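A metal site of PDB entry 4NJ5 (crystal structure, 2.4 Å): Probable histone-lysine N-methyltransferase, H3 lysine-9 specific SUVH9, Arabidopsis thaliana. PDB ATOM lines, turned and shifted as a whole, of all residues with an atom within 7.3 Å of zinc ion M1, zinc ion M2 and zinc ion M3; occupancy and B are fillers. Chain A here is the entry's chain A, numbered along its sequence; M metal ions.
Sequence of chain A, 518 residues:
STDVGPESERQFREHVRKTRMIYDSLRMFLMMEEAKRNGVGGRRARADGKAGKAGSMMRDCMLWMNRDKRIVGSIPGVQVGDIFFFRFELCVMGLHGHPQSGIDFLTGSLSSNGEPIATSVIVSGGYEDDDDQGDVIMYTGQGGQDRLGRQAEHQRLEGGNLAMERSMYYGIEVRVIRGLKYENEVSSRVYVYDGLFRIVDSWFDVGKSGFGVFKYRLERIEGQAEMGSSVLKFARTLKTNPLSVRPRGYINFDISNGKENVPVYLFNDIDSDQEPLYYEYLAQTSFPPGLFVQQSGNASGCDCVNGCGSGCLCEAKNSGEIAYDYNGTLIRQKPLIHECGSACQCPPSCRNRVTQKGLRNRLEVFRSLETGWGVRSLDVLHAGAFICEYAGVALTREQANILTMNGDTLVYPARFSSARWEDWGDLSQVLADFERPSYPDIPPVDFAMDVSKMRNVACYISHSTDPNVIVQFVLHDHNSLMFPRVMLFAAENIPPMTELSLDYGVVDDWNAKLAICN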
ATOM      1  N   SER A 300     -32.958  19.708 -12.608  1.00  0.00           N
ATOM      2  CA  SER A 300     -32.942  19.147 -11.268  1.00  0.00           C
ATOM      3  C   SER A 300     -31.524  19.116 -10.696  1.00  0.00           C
ATOM      4  O   SER A 300     -30.555  18.941 -11.439  1.00  0.00           O
ATOM      5  CB  SER A 300     -33.518  17.751 -11.321  1.00  0.00           C
ATOM      6  OG  SER A 300     -32.996  17.087 -12.446  1.00  0.00           O
ATOM      7  N   GLY A 301     -31.414  19.292  -9.384  1.00  0.00           N
ATOM      8  CA  GLY A 301     -30.127  19.286  -8.706  1.00  0.00           C
ATOM      9  C   GLY A 301     -30.018  18.110  -7.757  1.00  0.00           C
ATOM     10  O   GLY A 301     -31.018  17.465  -7.430  1.00  0.00           O
ATOM     11  N   CYS A 302     -28.796  17.815  -7.318  1.00  0.00           N
ATOM     12  CA  CYS A 302     -28.599  16.769  -6.333  1.00  0.00           C
ATOM     13  C   CYS A 302     -28.958  17.280  -4.935  1.00  0.00           C
ATOM     14  O   CYS A 302     -29.161  18.485  -4.731  1.00  0.00           O
ATOM     15  CB  CYS A 302     -27.172  16.228  -6.359  1.00  0.00           C
ATOM     16  SG  CYS A 302     -25.934  17.420  -5.852  1.00  0.00           S
ATOM     17  N   ASP A 303     -29.040  16.362  -3.983  1.00  0.00           N
ATOM     18  CA  ASP A 303     -29.461  16.689  -2.618  1.00  0.00           C
ATOM     19  C   ASP A 303     -28.361  16.439  -1.598  1.00  0.00           C
ATOM     20  O   ASP A 303     -28.629  16.020  -0.470  1.00  0.00           O
ATOM     21  CB  ASP A 303     -30.705  15.863  -2.252  1.00  0.00           C
ATOM     22  CG  ASP A 303     -30.480  14.368  -2.372  1.00  0.00           C
ATOM     23  OD1 ASP A 303     -29.383  13.963  -2.813  1.00  0.00           O
ATOM     24  OD2 ASP A 303     -31.403  13.600  -2.041  1.00  0.00           O
ATOM     25  N   CYS A 304     -27.114  16.701  -1.995  1.00  0.00           N
ATOM     26  CA  CYS A 304     -25.954  16.423  -1.160  1.00  0.00           C
ATOM     27  C   CYS A 304     -25.637  17.552  -0.192  1.00  0.00           C
ATOM     28  O   CYS A 304     -24.646  18.255  -0.361  1.00  0.00           O
ATOM     29  CB  CYS A 304     -24.727  16.129  -2.031  1.00  0.00           C
ATOM     30  SG  CYS A 304     -24.956  14.729  -3.134  1.00  0.00           S
ATOM     31  N   VAL A 305     -26.469  17.698   0.829  1.00  0.00           N
ATOM     32  CA  VAL A 305     -26.388  18.820   1.757  1.00  0.00           C
ATOM     33  C   VAL A 305     -25.057  18.946   2.501  1.00  0.00           C
ATOM     34  O   VAL A 305     -24.777  19.975   3.114  1.00  0.00           O
ATOM     35  CB  VAL A 305     -27.543  18.783   2.767  1.00  0.00           C
ATOM     36  CG1 VAL A 305     -28.875  18.838   2.035  1.00  0.00           C
ATOM     37  CG2 VAL A 305     -27.453  17.534   3.626  1.00  0.00           C
ATOM     38  N   GLY A 307     -22.127  18.160   0.701  1.00  0.00           N
ATOM     39  CA  GLY A 307     -21.172  18.084  -0.382  1.00  0.00           C
ATOM     40  C   GLY A 307     -21.306  16.787  -1.161  1.00  0.00           C
ATOM     41  O   GLY A 307     -21.630  15.748  -0.575  1.00  0.00           O
ATOM     42  N   CYS A 308     -21.074  16.842  -2.466  1.00  0.00           N
ATOM     43  CA  CYS A 308     -21.184  15.644  -3.292  1.00  0.00           C
ATOM     44  C   CYS A 308     -20.152  14.601  -2.896  1.00  0.00           C
ATOM     45  O   CYS A 308     -18.965  14.891  -2.816  1.00  0.00           O
ATOM     46  CB  CYS A 308     -21.041  15.973  -4.783  1.00  0.00           C
ATOM     47  SG  CYS A 308     -22.474  16.792  -5.508  1.00  0.00           S
ATOM     48  N   GLY A 309     -20.629  13.391  -2.644  1.00  0.00           N
ATOM     49  CA  GLY A 309     -19.755  12.254  -2.399  1.00  0.00           C
ATOM     50  C   GLY A 309     -19.888  11.265  -3.542  1.00  0.00           C
ATOM     51  O   GLY A 309     -19.399  11.523  -4.641  1.00  0.00           O
ATOM     52  N   SER A 310     -20.574  10.158  -3.295  1.00  0.00           N
ATOM     53  CA  SER A 310     -20.764   9.118  -4.303  1.00  0.00           C
ATOM     54  C   SER A 310     -22.231   8.717  -4.426  1.00  0.00           C
ATOM     55  O   SER A 310     -22.961   8.692  -3.437  1.00  0.00           O
ATOM     56  CB  SER A 310     -19.936   7.881  -3.971  1.00  0.00           C
ATOM     57  OG  SER A 310     -18.558   8.090  -4.255  1.00  0.00           O
ATOM     58  N   GLY A 311     -22.658   8.390  -5.645  1.00  0.00           N
ATOM     59  CA  GLY A 311     -23.977   7.843  -5.868  1.00  0.00           C
ATOM     60  C   GLY A 311     -25.112   8.831  -5.948  1.00  0.00           C
ATOM     61  O   GLY A 311     -26.279   8.455  -5.837  1.00  0.00           O
ATOM     62  N   CYS A 312     -24.797  10.116  -6.139  1.00  0.00           N
ATOM     63  CA  CYS A 312     -25.846  11.116  -6.289  1.00  0.00           C
ATOM     64  C   CYS A 312     -26.207  11.330  -7.761  1.00  0.00           C
ATOM     65  O   CYS A 312     -25.569  10.779  -8.662  1.00  0.00           O
ATOM     66  CB  CYS A 312     -25.447  12.433  -5.630  1.00  0.00           C
ATOM     67  SG  CYS A 312     -24.513  13.572  -6.681  1.00  0.00           S
ATOM     68  N   LEU A 313     -27.250  12.131  -7.987  1.00  0.00           N
ATOM     69  CA  LEU A 313     -27.755  12.400  -9.331  1.00  0.00           C
ATOM     70  C   LEU A 313     -26.711  13.062 -10.230  1.00  0.00           C
ATOM     71  O   LEU A 313     -26.549  12.677 -11.389  1.00  0.00           O
ATOM     72  CB  LEU A 313     -29.010  13.290  -9.241  1.00  0.00           C
ATOM     73  CG  LEU A 313     -29.279  14.282 -10.374  1.00  0.00           C
ATOM     74  CD1 LEU A 313     -29.750  13.579 -11.629  1.00  0.00           C
ATOM     75  CD2 LEU A 313     -30.268  15.350  -9.930  1.00  0.00           C
ATOM     76  N   CYS A 314     -26.009  14.050  -9.686  1.00  0.00           N
ATOM     77  CA  CYS A 314     -24.993  14.762 -10.448  1.00  0.00           C
ATOM     78  C   CYS A 314     -23.836  13.857 -10.872  1.00  0.00           C
ATOM     79  O   CYS A 314     -23.224  14.076 -11.916  1.00  0.00           O
ATOM     80  CB  CYS A 314     -24.495  15.976  -9.672  1.00  0.00           C
ATOM     81  SG  CYS A 314     -25.718  17.303  -9.588  1.00  0.00           S
ATOM     82  N   GLU A 315     -23.551  12.825 -10.077  1.00  0.00           N
ATOM     83  CA  GLU A 315     -22.571  11.831 -10.491  1.00  0.00           C
ATOM     84  C   GLU A 315     -23.083  11.039 -11.687  1.00  0.00           C
ATOM     85  O   GLU A 315     -22.347  10.753 -12.625  1.00  0.00           O
ATOM     86  CB  GLU A 315     -22.206  10.895  -9.342  1.00  0.00           C
ATOM     87  CG  GLU A 315     -21.252   9.786  -9.760  1.00  0.00           C
ATOM     88  CD  GLU A 315     -20.639   9.044  -8.587  1.00  0.00           C
ATOM     89  OE1 GLU A 315     -19.511   9.384  -8.198  1.00  0.00           O
ATOM     90  OE2 GLU A 315     -21.294   8.111  -8.057  1.00  0.00           O
ATOM     91  N   LYS A 317     -25.106  12.161 -13.872  1.00  0.00           N
ATOM     92  CA  LYS A 317     -25.030  13.093 -14.994  1.00  0.00           C
ATOM     93  C   LYS A 317     -23.629  13.087 -15.608  1.00  0.00           C
ATOM     94  O   LYS A 317     -23.460  13.361 -16.794  1.00  0.00           O
ATOM     95  CB  LYS A 317     -25.420  14.515 -14.570  1.00  0.00           C
ATOM     96  CG  LYS A 317     -26.830  14.640 -13.991  1.00  0.00           C
ATOM     97  CD  LYS A 317     -27.123  16.076 -13.515  1.00  0.00           C
ATOM     98  CE  LYS A 317     -27.326  17.027 -14.684  1.00  0.00           C
ATOM     99  NZ  LYS A 317     -27.064  18.448 -14.314  1.00  0.00           N
ATOM    100  N   ILE A 322     -17.791  11.858 -10.706  1.00  0.00           N
ATOM    101  CA  ILE A 322     -17.608  13.287 -10.476  1.00  0.00           C
ATOM    102  C   ILE A 322     -16.247  13.707 -11.015  1.00  0.00           C
ATOM    103  O   ILE A 322     -15.230  13.095 -10.716  1.00  0.00           O
ATOM    104  CB  ILE A 322     -17.687  13.624  -8.971  1.00  0.00           C
ATOM    105  CG1 ILE A 322     -19.043  13.208  -8.401  1.00  0.00           C
ATOM    106  CG2 ILE A 322     -17.466  15.113  -8.754  1.00  0.00           C
ATOM    107  CD1 ILE A 322     -20.190  14.115  -8.834  1.00  0.00           C
ATOM    108  N   HIS A 338     -20.582  18.241 -15.889  1.00  0.00           N
ATOM    109  CA  HIS A 338     -21.758  18.829 -15.244  1.00  0.00           C
ATOM    110  C   HIS A 338     -21.440  19.175 -13.790  1.00  0.00           C
ATOM    111  O   HIS A 338     -21.421  18.297 -12.924  1.00  0.00           O
ATOM    112  CB  HIS A 338     -22.951  17.864 -15.298  1.00  0.00           C
ATOM    113  CG  HIS A 338     -23.389  17.505 -16.682  1.00  0.00           C
ATOM    114  ND1 HIS A 338     -24.367  18.210 -17.363  1.00  0.00           N
ATOM    115  CD2 HIS A 338     -22.994  16.515 -17.515  1.00  0.00           C
ATOM    116  CE1 HIS A 338     -24.548  17.668 -18.550  1.00  0.00           C
ATOM    117  NE2 HIS A 338     -23.732  16.639 -18.675  1.00  0.00           N
ATOM    118  N   GLU A 339     -21.181  20.442 -13.530  1.00  0.00           N
ATOM    119  CA  GLU A 339     -20.973  20.907 -12.162  1.00  0.00           C
ATOM    120  C   GLU A 339     -22.320  21.137 -11.500  1.00  0.00           C
ATOM    121  O   GLU A 339     -23.334  21.287 -12.171  1.00  0.00           O
ATOM    122  CB  GLU A 339     -20.136  22.194 -12.135  1.00  0.00           C
ATOM    123  CG  GLU A 339     -18.651  21.953 -12.366  1.00  0.00           C
ATOM    124  CD  GLU A 339     -17.809  23.208 -12.201  1.00  0.00           C
ATOM    125  OE1 GLU A 339     -18.334  24.228 -11.706  1.00  0.00           O
ATOM    126  OE2 GLU A 339     -16.612  23.149 -12.568  1.00  0.00           O
ATOM    127  N   CYS A 340     -22.331  21.161 -10.167  1.00  0.00           N
ATOM    128  CA  CYS A 340     -23.551  21.467  -9.436  1.00  0.00           C
ATOM    129  C   CYS A 340     -23.936  22.927  -9.641  1.00  0.00           C
ATOM    130  O   CYS A 340     -23.065  23.790  -9.779  1.00  0.00           O
ATOM    131  CB  CYS A 340     -23.369  21.176  -7.951  1.00  0.00           C
ATOM    132  SG  CYS A 340     -23.012  19.453  -7.607  1.00  0.00           S
ATOM    133  N   GLY A 341     -25.231  23.184  -9.682  1.00  0.00           N
ATOM    134  CA  GLY A 341     -25.726  24.543  -9.850  1.00  0.00           C
ATOM    135  C   GLY A 341     -26.698  24.942  -8.755  1.00  0.00           C
ATOM    136  O   GLY A 341     -26.729  24.325  -7.684  1.00  0.00           O
ATOM    137  N   ALA A 343     -29.794  24.562  -8.534  1.00  0.00           N
ATOM    138  CA  ALA A 343     -30.777  23.524  -8.236  1.00  0.00           C
ATOM    139  C   ALA A 343     -30.228  22.487  -7.252  1.00  0.00           C
ATOM    140  O   ALA A 343     -30.987  21.765  -6.613  1.00  0.00           O
ATOM    141  CB  ALA A 343     -31.254  22.852  -9.518  1.00  0.00           C
ATOM    142  N   CYS A 344     -28.904  22.427  -7.116  1.00  0.00           N
ATOM    143  CA  CYS A 344     -28.293  21.509  -6.167  1.00  0.00           C
ATOM    144  C   CYS A 344     -28.291  22.056  -4.747  1.00  0.00           C
ATOM    145  O   CYS A 344     -28.222  23.274  -4.533  1.00  0.00           O
ATOM    146  CB  CYS A 344     -26.871  21.143  -6.605  1.00  0.00           C
ATOM    147  SG  CYS A 344     -26.805  20.321  -8.211  1.00  0.00           S
ATOM    148  N   GLN A 345     -28.370  21.157  -3.772  1.00  0.00           N
ATOM    149  CA  GLN A 345     -28.486  21.544  -2.372  1.00  0.00           C
ATOM    150  C   GLN A 345     -27.150  21.440  -1.647  1.00  0.00           C
ATOM    151  O   GLN A 345     -27.077  21.665  -0.439  1.00  0.00           O
ATOM    152  CB  GLN A 345     -29.554  20.706  -1.675  1.00  0.00           C
ATOM    153  CG  GLN A 345     -30.952  20.981  -2.187  1.00  0.00           C
ATOM    154  CD  GLN A 345     -31.967  19.975  -1.684  1.00  0.00           C
ATOM    155  OE1 GLN A 345     -31.925  18.799  -2.045  1.00  0.00           O
ATOM    156  NE2 GLN A 345     -32.893  20.424  -0.855  1.00  0.00           N
ATOM    157  N   CYS A 346     -26.097  21.100  -2.381  1.00  0.00           N
ATOM    158  CA  CYS A 346     -24.757  21.097  -1.815  1.00  0.00           C
ATOM    159  C   CYS A 346     -24.286  22.531  -1.605  1.00  0.00           C
ATOM    160  O   CYS A 346     -24.688  23.430  -2.346  1.00  0.00           O
ATOM    161  CB  CYS A 346     -23.790  20.315  -2.705  1.00  0.00           C
ATOM    162  SG  CYS A 346     -23.826  20.770  -4.442  1.00  0.00           S
ATOM    163  N   PRO A 347     -23.443  22.752  -0.584  1.00  0.00           N
ATOM    164  CA  PRO A 347     -22.870  24.072  -0.279  1.00  0.00           C
ATOM    165  C   PRO A 347     -21.777  24.436  -1.278  1.00  0.00           C
ATOM    166  O   PRO A 347     -21.399  23.601  -2.101  1.00  0.00           O
ATOM    167  CB  PRO A 347     -22.268  23.853   1.111  1.00  0.00           C
ATOM    168  CG  PRO A 347     -21.926  22.405   1.147  1.00  0.00           C
ATOM    169  CD  PRO A 347     -23.027  21.732   0.393  1.00  0.00           C
ATOM    170  N   SER A 349     -18.728  24.635  -0.846  1.00  0.00           N
ATOM    171  CA  SER A 349     -17.514  23.843  -0.631  1.00  0.00           C
ATOM    172  C   SER A 349     -17.536  22.487  -1.337  1.00  0.00           C
ATOM    173  O   SER A 349     -16.548  21.758  -1.304  1.00  0.00           O
ATOM    174  CB  SER A 349     -17.283  23.626   0.872  1.00  0.00           C
ATOM    175  OG  SER A 349     -18.213  22.696   1.385  1.00  0.00           O
ATOM    176  N   CYS A 350     -18.659  22.149  -1.958  1.00  0.00           N
ATOM    177  CA  CYS A 350     -18.780  20.883  -2.682  1.00  0.00           C
ATOM    178  C   CYS A 350     -17.699  20.724  -3.757  1.00  0.00           C
ATOM    179  O   CYS A 350     -17.388  21.668  -4.486  1.00  0.00           O
ATOM    180  CB  CYS A 350     -20.154  20.749  -3.317  1.00  0.00           C
ATOM    181  SG  CYS A 350     -20.270  19.365  -4.469  1.00  0.00           S
ATOM    182  N   ARG A 351     -17.145  19.528  -3.861  1.00  0.00           N
ATOM    183  CA  ARG A 351     -16.066  19.258  -4.819  1.00  0.00           C
ATOM    184  C   ARG A 351     -16.512  19.358  -6.276  1.00  0.00           C
ATOM    185  O   ARG A 351     -15.689  19.385  -7.184  1.00  0.00           O
ATOM    186  CB  ARG A 351     -15.445  17.878  -4.564  1.00  0.00           C
ATOM    187  CG  ARG A 351     -16.336  16.708  -4.969  1.00  0.00           C
ATOM    188  CD  ARG A 351     -15.616  15.379  -4.779  1.00  0.00           C
ATOM    189  NE  ARG A 351     -16.528  14.246  -4.877  1.00  0.00           N
ATOM    190  CZ  ARG A 351     -16.365  13.229  -5.712  1.00  0.00           C
ATOM    191  NH1 ARG A 351     -15.328  13.188  -6.530  1.00  0.00           N
ATOM    192  NH2 ARG A 351     -17.241  12.231  -5.723  1.00  0.00           N
ATOM    193  N   ASN A 352     -17.817  19.406  -6.514  1.00  0.00           N
ATOM    194  CA  ASN A 352     -18.320  19.497  -7.881  1.00  0.00           C
ATOM    195  C   ASN A 352     -18.681  20.927  -8.272  1.00  0.00           C
ATOM    196  O   ASN A 352     -19.586  21.155  -9.085  1.00  0.00           O
ATOM    197  CB  ASN A 352     -19.506  18.547  -8.095  1.00  0.00           C
ATOM    198  CG  ASN A 352     -19.718  18.216  -9.557  1.00  0.00           C
ATOM    199  OD1 ASN A 352     -18.767  18.203 -10.340  1.00  0.00           O
ATOM    200  ND2 ASN A 352     -20.963  17.951  -9.926  1.00  0.00           N
ATOM    201  N   ARG A 353     -17.977  21.896  -7.689  1.00  0.00           N
ATOM    202  CA  ARG A 353     -18.190  23.304  -8.004  1.00  0.00           C
ATOM    203  C   ARG A 353     -16.874  24.024  -8.283  1.00  0.00           C
ATOM    204  O   ARG A 353     -16.643  25.124  -7.792  1.00  0.00           O
ATOM    205  CB  ARG A 353     -18.937  24.005  -6.852  1.00  0.00           C
ATOM    206  CG  ARG A 353     -20.360  23.530  -6.612  1.00  0.00           C
ATOM    207  CD  ARG A 353     -21.044  24.356  -5.536  1.00  0.00           C
ATOM    208  NE  ARG A 353     -22.401  23.900  -5.223  1.00  0.00           N
ATOM    209  CZ  ARG A 353     -23.495  24.324  -5.838  1.00  0.00           C
ATOM    210  NH1 ARG A 353     -23.404  25.205  -6.826  1.00  0.00           N
ATOM    211  NH2 ARG A 353     -24.684  23.862  -5.487  1.00  0.00           N
HETATM  212 ZN    ZN M   1     -25.193  18.560  -7.738  1.00  0.00          ZN
HETATM  213 ZN    ZN M   2     -22.468  19.075  -5.300  1.00  0.00          ZN
HETATM  214 ZN    ZN M   3     -24.359  15.507  -5.217  1.00  0.00          ZN
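Zinc ion M1 is bound by the side-chain sulfur (SG) of Cys 314, the side-chain sulfur (SG) of Cys 302, the side-chain sulfur (SG) of Cys 340 and the side-chain sulfur (SG) of Cys 344.
Zinc ion M2 is bound by SG of Cys 308 (2.3 Å), SG of Cys 346 (2.3 Å), SG of Cys 350 (2.4 Å) and SG of Cys 340 (2.4 Å). Zinc ion M2 has four donor atoms within binding distance.
The guanidinium group of Arg 351 is in hydrogen-bond range of the backbone carbonyl oxygen of Cys 308 (3.3 Å). The backbone NH (N) of Cys 314 sits close to the side-chain sulfur (SG) of Cys 312, at 3.4 Å. The backbone NH of Gln 345 is in hydrogen-bond range of the backbone carbonyl oxygen of Cys 302. The guanidinium group (NH2) of Arg 353 sits at hydrogen-bond distance from the backbone carbonyl oxygen (O) of Cys 346 (3.2 Å). N of Cys 340 is in hydrogen-bond range of O of Asn 352 (3.0 Å). O of Cys 340 is in hydrogen-bond range of NH1 of Arg 353. The backbone NH (N) of Glu 315 sits close to the side-chain sulfur (SG) of Cys 312, at 3.6 Å. The side-chain sulfur (SG) of Cys 344 lies close to the backbone NH (N) of Gly 341.
Five residues have an atom within 4 Å of zinc ion M2: Cys 302, Cys 308, Cys 340, Cys 346 and Cys 350. The nearest printed residue that does not touch zinc ion M2 is Asn 352 (4.1 Å).
Of the 31 residues printed, 4 come within 4 Å of zinc ion M3.
Zinc ion M3 is bound by the side-chain sulfur (SG) of Cys 308 (2.3 Å). The side-chain sulfur (SG) of Cys 304 is bound to zinc ion M3, 2.3 Å away. The side-chain sulfur (SG) of Cys 312 binds zinc ion M3, 2.4 Å away. SG of Cys 302 binds zinc ion M3 (2.6 Å).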
